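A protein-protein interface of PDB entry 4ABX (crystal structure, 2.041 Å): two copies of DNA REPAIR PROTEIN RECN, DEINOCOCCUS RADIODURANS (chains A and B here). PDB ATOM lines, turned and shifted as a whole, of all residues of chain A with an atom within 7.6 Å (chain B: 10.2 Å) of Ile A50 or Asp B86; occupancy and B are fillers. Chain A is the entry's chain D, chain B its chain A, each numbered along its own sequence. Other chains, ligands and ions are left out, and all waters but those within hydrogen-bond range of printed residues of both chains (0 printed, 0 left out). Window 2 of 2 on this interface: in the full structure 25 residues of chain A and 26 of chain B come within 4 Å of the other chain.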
ATOM      1  N   ARG A  43      -8.700  32.958 -12.489  1.00  0.00           N
ATOM      2  CA  ARG A  43      -9.088  32.036 -13.557  1.00  0.00           C
ATOM      3  C   ARG A  43      -7.914  31.183 -14.014  1.00  0.00           C
ATOM      4  O   ARG A  43      -8.041  29.967 -14.163  1.00  0.00           O
ATOM      5  CB  ARG A  43      -9.647  32.785 -14.767  1.00  0.00           C
ATOM      6  CG  ARG A  43     -10.082  31.850 -15.899  1.00  0.00           C
ATOM      7  CD  ARG A  43     -10.561  32.605 -17.138  1.00  0.00           C
ATOM      8  NE  ARG A  43      -9.466  33.276 -17.826  1.00  0.00           N
ATOM      9  CZ  ARG A  43      -8.680  32.695 -18.727  1.00  0.00           C
ATOM     10  NH1 ARG A  43      -8.868  31.425 -19.062  1.00  0.00           N
ATOM     11  NH2 ARG A  43      -7.706  33.385 -19.297  1.00  0.00           N
ATOM     12  N   LEU A  44      -6.777  31.828 -14.259  1.00  0.00           N
ATOM     13  CA  LEU A  44      -5.584  31.128 -14.713  1.00  0.00           C
ATOM     14  C   LEU A  44      -4.965  30.291 -13.598  1.00  0.00           C
ATOM     15  O   LEU A  44      -4.495  29.176 -13.832  1.00  0.00           O
ATOM     16  CB  LEU A  44      -4.562  32.117 -15.274  1.00  0.00           C
ATOM     17  CG  LEU A  44      -5.002  32.788 -16.578  1.00  0.00           C
ATOM     18  CD1 LEU A  44      -4.185  34.039 -16.844  1.00  0.00           C
ATOM     19  CD2 LEU A  44      -4.902  31.813 -17.741  1.00  0.00           C
ATOM     20  N   SER A  45      -4.951  30.830 -12.388  1.00  0.00           N
ATOM     21  CA  SER A  45      -4.437  30.066 -11.256  1.00  0.00           C
ATOM     22  C   SER A  45      -5.260  28.791 -11.068  1.00  0.00           C
ATOM     23  O   SER A  45      -4.704  27.698 -10.945  1.00  0.00           O
ATOM     24  CB  SER A  45      -4.450  30.900  -9.976  1.00  0.00           C
ATOM     25  OG  SER A  45      -3.759  30.229  -8.934  1.00  0.00           O
ATOM     26  N   ASN A  46      -6.582  28.934 -11.054  1.00  0.00           N
ATOM     27  CA  ASN A  46      -7.462  27.787 -10.880  1.00  0.00           C
ATOM     28  C   ASN A  46      -7.290  26.747 -11.984  1.00  0.00           C
ATOM     29  O   ASN A  46      -7.273  25.549 -11.715  1.00  0.00           O
ATOM     30  CB  ASN A  46      -8.921  28.222 -10.765  1.00  0.00           C
ATOM     31  CG  ASN A  46      -9.193  29.016  -9.502  1.00  0.00           C
ATOM     32  OD1 ASN A  46      -8.344  29.096  -8.614  1.00  0.00           O
ATOM     33  ND2 ASN A  46     -10.381  29.611  -9.417  1.00  0.00           N
ATOM     34  N   LEU A  47      -7.144  27.208 -13.223  1.00  0.00           N
ATOM     35  CA  LEU A  47      -6.898  26.293 -14.333  1.00  0.00           C
ATOM     36  C   LEU A  47      -5.716  25.379 -14.038  1.00  0.00           C
ATOM     37  O   LEU A  47      -5.778  24.171 -14.266  1.00  0.00           O
ATOM     38  CB  LEU A  47      -6.664  27.056 -15.641  1.00  0.00           C
ATOM     39  CG  LEU A  47      -7.919  27.487 -16.398  1.00  0.00           C
ATOM     40  CD1 LEU A  47      -7.550  28.189 -17.702  1.00  0.00           C
ATOM     41  CD2 LEU A  47      -8.829  26.288 -16.665  1.00  0.00           C
ATOM     42  N   HIS A  48      -4.638  25.964 -13.530  1.00  0.00           N
ATOM     43  CA  HIS A  48      -3.452  25.195 -13.176  1.00  0.00           C
ATOM     44  C   HIS A  48      -3.761  24.193 -12.065  1.00  0.00           C
ATOM     45  O   HIS A  48      -3.350  23.036 -12.123  1.00  0.00           O
ATOM     46  CB  HIS A  48      -2.327  26.128 -12.728  1.00  0.00           C
ATOM     47  CG  HIS A  48      -1.116  25.405 -12.226  1.00  0.00           C
ATOM     48  ND1 HIS A  48      -0.082  25.023 -13.049  1.00  0.00           N
ATOM     49  CD2 HIS A  48      -0.789  24.976 -10.983  1.00  0.00           C
ATOM     50  CE1 HIS A  48       0.837  24.398 -12.339  1.00  0.00           C
ATOM     51  NE2 HIS A  48       0.434  24.357 -11.079  1.00  0.00           N
ATOM     52  N   THR A  49      -4.485  24.651 -11.049  1.00  0.00           N
ATOM     53  CA  THR A  49      -4.879  23.785  -9.947  1.00  0.00           C
ATOM     54  C   THR A  49      -5.701  22.589 -10.445  1.00  0.00           C
ATOM     55  O   THR A  49      -5.467  21.450 -10.036  1.00  0.00           O
ATOM     56  CB  THR A  49      -5.663  24.576  -8.886  1.00  0.00           C
ATOM     57  OG1 THR A  49      -4.808  25.584  -8.322  1.00  0.00           O
ATOM     58  CG2 THR A  49      -6.156  23.658  -7.783  1.00  0.00           C
ATOM     59  N   ILE A  50      -6.654  22.853 -11.328  1.00  0.00           N
ATOM     60  CA  ILE A  50      -7.483  21.797 -11.912  1.00  0.00           C
ATOM     61  C   ILE A  50      -6.636  20.764 -12.656  1.00  0.00           C
ATOM     62  O   ILE A  50      -6.847  19.557 -12.517  1.00  0.00           O
ATOM     63  CB  ILE A  50      -8.539  22.383 -12.877  1.00  0.00           C
ATOM     64  CG1 ILE A  50      -9.544  23.247 -12.111  1.00  0.00           C
ATOM     65  CG2 ILE A  50      -9.270  21.273 -13.620  1.00  0.00           C
ATOM     66  CD1 ILE A  50     -10.333  24.191 -12.992  1.00  0.00           C
ATOM     67  N   ALA A  51      -5.673  21.238 -13.442  1.00  0.00           N
ATOM     68  CA  ALA A  51      -4.830  20.343 -14.229  1.00  0.00           C
ATOM     69  C   ALA A  51      -3.946  19.460 -13.344  1.00  0.00           C
ATOM     70  O   ALA A  51      -3.766  18.271 -13.622  1.00  0.00           O
ATOM     71  CB  ALA A  51      -3.979  21.139 -15.220  1.00  0.00           C
ATOM     72  N   GLN A  52      -3.394  20.042 -12.283  1.00  0.00           N
ATOM     73  CA  GLN A  52      -2.559  19.284 -11.352  1.00  0.00           C
ATOM     74  C   GLN A  52      -3.362  18.245 -10.565  1.00  0.00           C
ATOM     75  O   GLN A  52      -2.852  17.182 -10.222  1.00  0.00           O
ATOM     76  CB  GLN A  52      -1.823  20.219 -10.387  1.00  0.00           C
ATOM     77  CG  GLN A  52      -0.774  21.080 -11.060  1.00  0.00           C
ATOM     78  CD  GLN A  52       0.344  21.473 -10.116  1.00  0.00           C
ATOM     79  OE1 GLN A  52       1.510  21.145 -10.348  1.00  0.00           O
ATOM     80  NE2 GLN A  52      -0.004  22.178  -9.045  1.00  0.00           N
ATOM     81  N   ALA A  53      -4.616  18.566 -10.270  1.00  0.00           N
ATOM     82  CA  ALA A  53      -5.483  17.652  -9.544  1.00  0.00           C
ATOM     83  C   ALA A  53      -5.825  16.438 -10.411  1.00  0.00           C
ATOM     84  O   ALA A  53      -5.723  15.290  -9.966  1.00  0.00           O
ATOM     85  CB  ALA A  53      -6.744  18.369  -9.109  1.00  0.00           C
ATOM     86  N   ALA A  54      -6.222  16.694 -11.652  1.00  0.00           N
ATOM     87  CA  ALA A  54      -6.548  15.611 -12.572  1.00  0.00           C
ATOM     88  C   ALA A  54      -5.351  14.678 -12.764  1.00  0.00           C
ATOM     89  O   ALA A  54      -5.502  13.455 -12.748  1.00  0.00           O
ATOM     90  CB  ALA A  54      -7.023  16.161 -13.910  1.00  0.00           C
ATOM     91  N   ALA A  55      -4.166  15.257 -12.928  1.00  0.00           N
ATOM     92  CA  ALA A  55      -2.948  14.469 -13.117  1.00  0.00           C
ATOM     93  C   ALA A  55      -2.605  13.660 -11.871  1.00  0.00           C
ATOM     94  O   ALA A  55      -2.157  12.522 -11.966  1.00  0.00           O
ATOM     95  CB  ALA A  55      -1.784  15.366 -13.511  1.00  0.00           C
ATOM     96  N   GLY A  56      -2.815  14.250 -10.700  1.00  0.00           N
ATOM     97  CA  GLY A  56      -2.589  13.544  -9.455  1.00  0.00           C
ATOM     98  C   GLY A  56      -3.498  12.333  -9.318  1.00  0.00           C
ATOM     99  O   GLY A  56      -3.079  11.283  -8.830  1.00  0.00           O
ATOM    100  N   LEU A 110     -10.071  11.895 -16.665  1.00  0.00           N
ATOM    101  CA  LEU A 110      -9.206  12.814 -15.935  1.00  0.00           C
ATOM    102  C   LEU A 110      -8.000  13.163 -16.803  1.00  0.00           C
ATOM    103  O   LEU A 110      -7.552  14.304 -16.836  1.00  0.00           O
ATOM    104  CB  LEU A 110      -8.763  12.205 -14.604  1.00  0.00           C
ATOM    105  CG  LEU A 110      -9.830  12.221 -13.503  1.00  0.00           C
ATOM    106  CD1 LEU A 110      -9.365  11.417 -12.292  1.00  0.00           C
ATOM    107  CD2 LEU A 110     -10.176  13.653 -13.108  1.00  0.00           C
ATOM    108  N   VAL A 113      -8.927  15.851 -19.162  1.00  0.00           N
ATOM    109  CA  VAL A 113      -8.938  17.147 -18.492  1.00  0.00           C
ATOM    110  C   VAL A 113      -7.538  17.744 -18.463  1.00  0.00           C
ATOM    111  O   VAL A 113      -7.318  18.854 -18.946  1.00  0.00           O
ATOM    112  CB  VAL A 113      -9.478  17.055 -17.046  1.00  0.00           C
ATOM    113  CG1 VAL A 113      -9.275  18.386 -16.323  1.00  0.00           C
ATOM    114  CG2 VAL A 113     -10.948  16.656 -17.049  1.00  0.00           C
ATOM    115  N   ALA A 114      -6.591  16.998 -17.903  1.00  0.00           N
ATOM    116  CA  ALA A 114      -5.207  17.451 -17.831  1.00  0.00           C
ATOM    117  C   ALA A 114      -4.618  17.759 -19.214  1.00  0.00           C
ATOM    118  O   ALA A 114      -3.937  18.771 -19.394  1.00  0.00           O
ATOM    119  CB  ALA A 114      -4.347  16.426 -17.098  1.00  0.00           C
ATOM    120  N   SER A 117      -6.181  20.908 -21.015  1.00  0.00           N
ATOM    121  CA  SER A 117      -6.176  22.104 -20.175  1.00  0.00           C
ATOM    122  C   SER A 117      -5.777  23.369 -20.935  1.00  0.00           C
ATOM    123  O   SER A 117      -4.872  23.353 -21.769  1.00  0.00           O
ATOM    124  CB  SER A 117      -5.254  21.917 -18.966  1.00  0.00           C
ATOM    125  OG  SER A 117      -5.134  23.129 -18.233  1.00  0.00           O
ATOM    126  N   ALA A 119      -4.631  25.901 -19.276  1.00  0.00           N
ATOM    127  CA  ALA A 119      -3.710  26.572 -18.365  1.00  0.00           C
ATOM    128  C   ALA A 119      -2.597  27.217 -19.180  1.00  0.00           C
ATOM    129  O   ALA A 119      -2.068  26.608 -20.111  1.00  0.00           O
ATOM    130  CB  ALA A 119      -3.135  25.592 -17.351  1.00  0.00           C
ATOM    131  N   ALA B  78      -7.015  13.814  -3.763  1.00  0.00           N
ATOM    132  CA  ALA B  78      -6.226  14.538  -4.756  1.00  0.00           C
ATOM    133  C   ALA B  78      -7.108  15.408  -5.653  1.00  0.00           C
ATOM    134  O   ALA B  78      -6.673  16.445  -6.150  1.00  0.00           O
ATOM    135  CB  ALA B  78      -5.407  13.564  -5.593  1.00  0.00           C
ATOM    136  N   LEU B  79      -8.351  14.984  -5.856  1.00  0.00           N
ATOM    137  CA  LEU B  79      -9.278  15.720  -6.710  1.00  0.00           C
ATOM    138  C   LEU B  79      -9.938  16.922  -6.021  1.00  0.00           C
ATOM    139  O   LEU B  79     -10.509  17.784  -6.692  1.00  0.00           O
ATOM    140  CB  LEU B  79     -10.353  14.777  -7.263  1.00  0.00           C
ATOM    141  CG  LEU B  79      -9.824  13.676  -8.180  1.00  0.00           C
ATOM    142  CD1 LEU B  79     -10.975  12.895  -8.788  1.00  0.00           C
ATOM    143  CD2 LEU B  79      -8.945  14.280  -9.269  1.00  0.00           C
ATOM    144  N   ASN B  80      -9.856  16.984  -4.694  1.00  0.00           N
ATOM    145  CA  ASN B  80     -10.505  18.058  -3.932  1.00  0.00           C
ATOM    146  C   ASN B  80     -10.283  19.461  -4.496  1.00  0.00           C
ATOM    147  O   ASN B  80     -11.238  20.202  -4.732  1.00  0.00           O
ATOM    148  CB  ASN B  80     -10.071  18.034  -2.458  1.00  0.00           C
ATOM    149  CG  ASN B  80     -10.874  17.053  -1.624  1.00  0.00           C
ATOM    150  OD1 ASN B  80     -10.396  16.553  -0.602  1.00  0.00           O
ATOM    151  ND2 ASN B  80     -12.100  16.770  -2.052  1.00  0.00           N
ATOM    152  N   ALA B  81      -9.022  19.827  -4.704  1.00  0.00           N
ATOM    153  CA  ALA B  81      -8.686  21.192  -5.104  1.00  0.00           C
ATOM    154  C   ALA B  81      -9.216  21.509  -6.499  1.00  0.00           C
ATOM    155  O   ALA B  81      -9.618  22.638  -6.780  1.00  0.00           O
ATOM    156  CB  ALA B  81      -7.173  21.420  -5.034  1.00  0.00           C
ATOM    157  N   GLY B  82      -9.225  20.504  -7.369  1.00  0.00           N
ATOM    158  CA  GLY B  82      -9.734  20.687  -8.713  1.00  0.00           C
ATOM    159  C   GLY B  82     -11.249  20.758  -8.750  1.00  0.00           C
ATOM    160  O   GLY B  82     -11.831  21.518  -9.540  1.00  0.00           O
ATOM    161  N   ALA B  83     -11.893  19.977  -7.887  1.00  0.00           N
ATOM    162  CA  ALA B  83     -13.352  19.894  -7.887  1.00  0.00           C
ATOM    163  C   ALA B  83     -13.980  21.211  -7.458  1.00  0.00           C
ATOM    164  O   ALA B  83     -15.128  21.499  -7.794  1.00  0.00           O
ATOM    165  CB  ALA B  83     -13.834  18.745  -6.988  1.00  0.00           C
ATOM    166  N   LYS B  84     -13.220  22.003  -6.709  1.00  0.00           N
ATOM    167  CA  LYS B  84     -13.692  23.293  -6.215  1.00  0.00           C
ATOM    168  C   LYS B  84     -14.039  24.249  -7.352  1.00  0.00           C
ATOM    169  O   LYS B  84     -14.874  25.144  -7.189  1.00  0.00           O
ATOM    170  CB  LYS B  84     -12.621  23.956  -5.335  1.00  0.00           C
ATOM    171  CG  LYS B  84     -12.330  23.239  -4.032  1.00  0.00           C
ATOM    172  CD  LYS B  84     -11.305  24.008  -3.211  1.00  0.00           C
ATOM    173  CE  LYS B  84     -11.142  23.398  -1.828  1.00  0.00           C
ATOM    174  NZ  LYS B  84      -9.987  23.988  -1.091  1.00  0.00           N
ATOM    175  N   TYR B  85     -13.380  24.073  -8.494  1.00  0.00           N
ATOM    176  CA  TYR B  85     -13.441  25.063  -9.570  1.00  0.00           C
ATOM    177  C   TYR B  85     -13.944  24.471 -10.877  1.00  0.00           C
ATOM    178  O   TYR B  85     -14.263  25.202 -11.808  1.00  0.00           O
ATOM    179  CB  TYR B  85     -12.060  25.704  -9.786  1.00  0.00           C
ATOM    180  CG  TYR B  85     -11.397  26.104  -8.491  1.00  0.00           C
ATOM    181  CD1 TYR B  85     -11.905  27.149  -7.728  1.00  0.00           C
ATOM    182  CD2 TYR B  85     -10.284  25.419  -8.011  1.00  0.00           C
ATOM    183  CE1 TYR B  85     -11.324  27.512  -6.538  1.00  0.00           C
ATOM    184  CE2 TYR B  85      -9.691  25.777  -6.814  1.00  0.00           C
ATOM    185  CZ  TYR B  85     -10.222  26.824  -6.079  1.00  0.00           C
ATOM    186  OH  TYR B  85      -9.652  27.195  -4.888  1.00  0.00           O
ATOM    187  N   ASP B  86     -14.024  23.148 -10.957  1.00  0.00           N
ATOM    188  CA  ASP B  86     -14.411  22.537 -12.220  1.00  0.00           C
ATOM    189  C   ASP B  86     -15.536  21.516 -12.085  1.00  0.00           C
ATOM    190  O   ASP B  86     -15.413  20.530 -11.357  1.00  0.00           O
ATOM    191  CB  ASP B  86     -13.195  21.938 -12.927  1.00  0.00           C
ATOM    192  CG  ASP B  86     -13.538  21.396 -14.297  1.00  0.00           C
ATOM    193  OD1 ASP B  86     -13.654  22.198 -15.243  1.00  0.00           O
ATOM    194  OD2 ASP B  86     -13.708  20.169 -14.423  1.00  0.00           O
ATOM    195  N   GLU B  87     -16.632  21.767 -12.794  1.00  0.00           N
ATOM    196  CA  GLU B  87     -17.814  20.910 -12.725  1.00  0.00           C
ATOM    197  C   GLU B  87     -17.502  19.484 -13.167  1.00  0.00           C
ATOM    198  O   GLU B  87     -17.969  18.520 -12.556  1.00  0.00           O
ATOM    199  CB  GLU B  87     -18.952  21.499 -13.566  1.00  0.00           C
ATOM    200  CG  GLU B  87     -20.342  21.033 -13.148  1.00  0.00           C
ATOM    201  CD  GLU B  87     -21.430  22.044 -13.500  1.00  0.00           C
ATOM    202  OE1 GLU B  87     -21.566  22.381 -14.698  1.00  0.00           O
ATOM    203  OE2 GLU B  87     -22.143  22.507 -12.577  1.00  0.00           O
ATOM    204  N   THR B  88     -16.703  19.354 -14.222  1.00  0.00           N
ATOM    205  CA  THR B  88     -16.335  18.043 -14.748  1.00  0.00           C
ATOM    206  C   THR B  88     -15.477  17.237 -13.765  1.00  0.00           C
ATOM    207  O   THR B  88     -15.737  16.054 -13.537  1.00  0.00           O
ATOM    208  CB  THR B  88     -15.623  18.155 -16.114  1.00  0.00           C
ATOM    209  OG1 THR B  88     -16.529  18.710 -17.074  1.00  0.00           O
ATOM    210  CG2 THR B  88     -15.168  16.781 -16.601  1.00  0.00           C
ATOM    211  N   VAL B  89     -14.457  17.868 -13.191  1.00  0.00           N
ATOM    212  CA  VAL B  89     -13.663  17.212 -12.152  1.00  0.00           C
ATOM    213  C   VAL B  89     -14.544  16.837 -10.954  1.00  0.00           C
ATOM    214  O   VAL B  89     -14.457  15.726 -10.437  1.00  0.00           O
ATOM    215  CB  VAL B  89     -12.463  18.074 -11.697  1.00  0.00           C
ATOM    216  CG1 VAL B  89     -11.791  17.475 -10.468  1.00  0.00           C
ATOM    217  CG2 VAL B  89     -11.451  18.214 -12.829  1.00  0.00           C
ATOM    218  N   MET B  90     -15.404  17.758 -10.526  1.00  0.00           N
ATOM    219  CA  MET B  90     -16.303  17.475  -9.413  1.00  0.00           C
ATOM    220  C   MET B  90     -17.150  16.231  -9.700  1.00  0.00           C
ATOM    221  O   MET B  90     -17.295  15.352  -8.844  1.00  0.00           O
ATOM    222  CB  MET B  90     -17.200  18.675  -9.097  1.00  0.00           C
ATOM    223  CG  MET B  90     -18.352  18.334  -8.147  1.00  0.00           C
ATOM    224  SD  MET B  90     -19.299  19.758  -7.560  1.00  0.00           S
ATOM    225  CE  MET B  90     -18.035  20.644  -6.635  1.00  0.00           C
ATOM    226  N   GLN B  91     -17.689  16.147 -10.911  1.00  0.00           N
ATOM    227  CA  GLN B  91     -18.503  14.993 -11.293  1.00  0.00           C
ATOM    228  C   GLN B  91     -17.716  13.679 -11.264  1.00  0.00           C
ATOM    229  O   GLN B  91     -18.179  12.685 -10.706  1.00  0.00           O
ATOM    230  CB  GLN B  91     -19.134  15.196 -12.671  1.00  0.00           C
ATOM    231  CG  GLN B  91     -19.988  14.022 -13.121  1.00  0.00           C
ATOM    232  CD  GLN B  91     -20.880  14.365 -14.297  1.00  0.00           C
ATOM    233  OE1 GLN B  91     -21.211  15.532 -14.522  1.00  0.00           O
ATOM    234  NE2 GLN B  91     -21.276  13.348 -15.057  1.00  0.00           N
ATOM    235  N   LEU B  92     -16.532  13.678 -11.872  1.00  0.00           N
ATOM    236  CA  LEU B  92     -15.672  12.501 -11.861  1.00  0.00           C
ATOM    237  C   LEU B  92     -15.308  12.087 -10.436  1.00  0.00           C
ATOM    238  O   LEU B  92     -15.239  10.898 -10.128  1.00  0.00           O
ATOM    239  CB  LEU B  92     -14.400  12.750 -12.676  1.00  0.00           C
ATOM    240  CG  LEU B  92     -14.574  12.908 -14.184  1.00  0.00           C
ATOM    241  CD1 LEU B  92     -13.318  13.517 -14.814  1.00  0.00           C
ATOM    242  CD2 LEU B  92     -14.925  11.569 -14.830  1.00  0.00           C
ATOM    243  N   GLN B  93     -15.081  13.066  -9.564  1.00  0.00           N
ATOM    244  CA  GLN B  93     -14.790  12.777  -8.163  1.00  0.00           C
ATOM    245  C   GLN B  93     -15.953  12.045  -7.502  1.00  0.00           C
ATOM    246  O   GLN B  93     -15.754  11.091  -6.741  1.00  0.00           O
ATOM    247  CB  GLN B  93     -14.478  14.054  -7.376  1.00  0.00           C
ATOM    248  CG  GLN B  93     -13.933  13.777  -5.972  1.00  0.00           C
ATOM    249  CD  GLN B  93     -13.922  15.006  -5.083  1.00  0.00           C
ATOM    250  OE1 GLN B  93     -14.775  15.881  -5.206  1.00  0.00           O
ATOM    251  NE2 GLN B  93     -12.949  15.076  -4.182  1.00  0.00           N
ATOM    252  N   ASN B  94     -17.169  12.499  -7.788  1.00  0.00           N
ATOM    253  CA  ASN B  94     -18.365  11.850  -7.258  1.00  0.00           C
ATOM    254  C   ASN B  94     -18.543  10.432  -7.799  1.00  0.00           C
ATOM    255  O   ASN B  94     -18.885   9.517  -7.055  1.00  0.00           O
ATOM    256  CB  ASN B  94     -19.610  12.697  -7.528  1.00  0.00           C
ATOM    257  CG  ASN B  94     -19.718  13.892  -6.595  1.00  0.00           C
ATOM    258  OD1 ASN B  94     -20.164  14.967  -6.994  1.00  0.00           O
ATOM    259  ND2 ASN B  94     -19.318  13.704  -5.340  1.00  0.00           N
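Of the 17 printed residues of chain B, 8 touch a printed residue of chain A.
Of the 19 printed residues of chain A, 5 touch a printed residue of chain B.
Among the printed residues, no Asp or Glu carboxylate lies within 4 Å of a Lys or Arg side-chain nitrogen of the other chain.
CD1 of Tyr B85 touches ND2 of Asn A46, 3.4 Å away.
CG2 of Thr A49 touches CB of Ala B81, at 3.7 Å.
CG1 of Ile A50 touches O of Gly B82 (3.9 Å).
Ile A50 touches Tyr B85.
Ile A50 touches Asp B86 (CD1 to CB, 3.6 Å).
Val B89 touches Ile A50 (CG2 to CG2, 3.8 Å).
O of Ala B78 touches CB of Ala A53 (3.5 Å).
CD2 of Leu B79 touches O of Ala A53, at 3.4 Å.
Gly B82 touches Ala A53.
Leu A110 touches Leu B92 (CD2 to CD1, 3.6 Å).
No position is printed for both chains.
Of the 10 pairs that touch across the chains among the printed residues, none has its exchanged pair printed and touching as well.
Ile A50 touches four residues of chain B.
Of chain A, only Ile A50 comes within 4 Å of Asp B86.
Of chain B, only Ala B81 (3.7 Å) comes within 4 Å of Thr A49.
Ala A51 touches none of the printed residues of chain B.
Of the printed residues of chain B, Ala A53 touches Ala B78, Leu B79 and Gly B82.
Of the printed residues of chain A, Gly B82 touches Ile A50 and Ala A53.
Printed residues of chain B within 4 Å of Leu A110: Leu B92.
N of Thr B88 lies within hydrogen-bond range of OD2 of Asp B86.
The side-chain carboxylate of Asp B86 sits at hydrogen-bond distance from the backbone NH of Val B89, 2.7 Å away.
O of Ser A45 sits at hydrogen-bond distance from OG1 of Thr A49 (3.4 Å).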
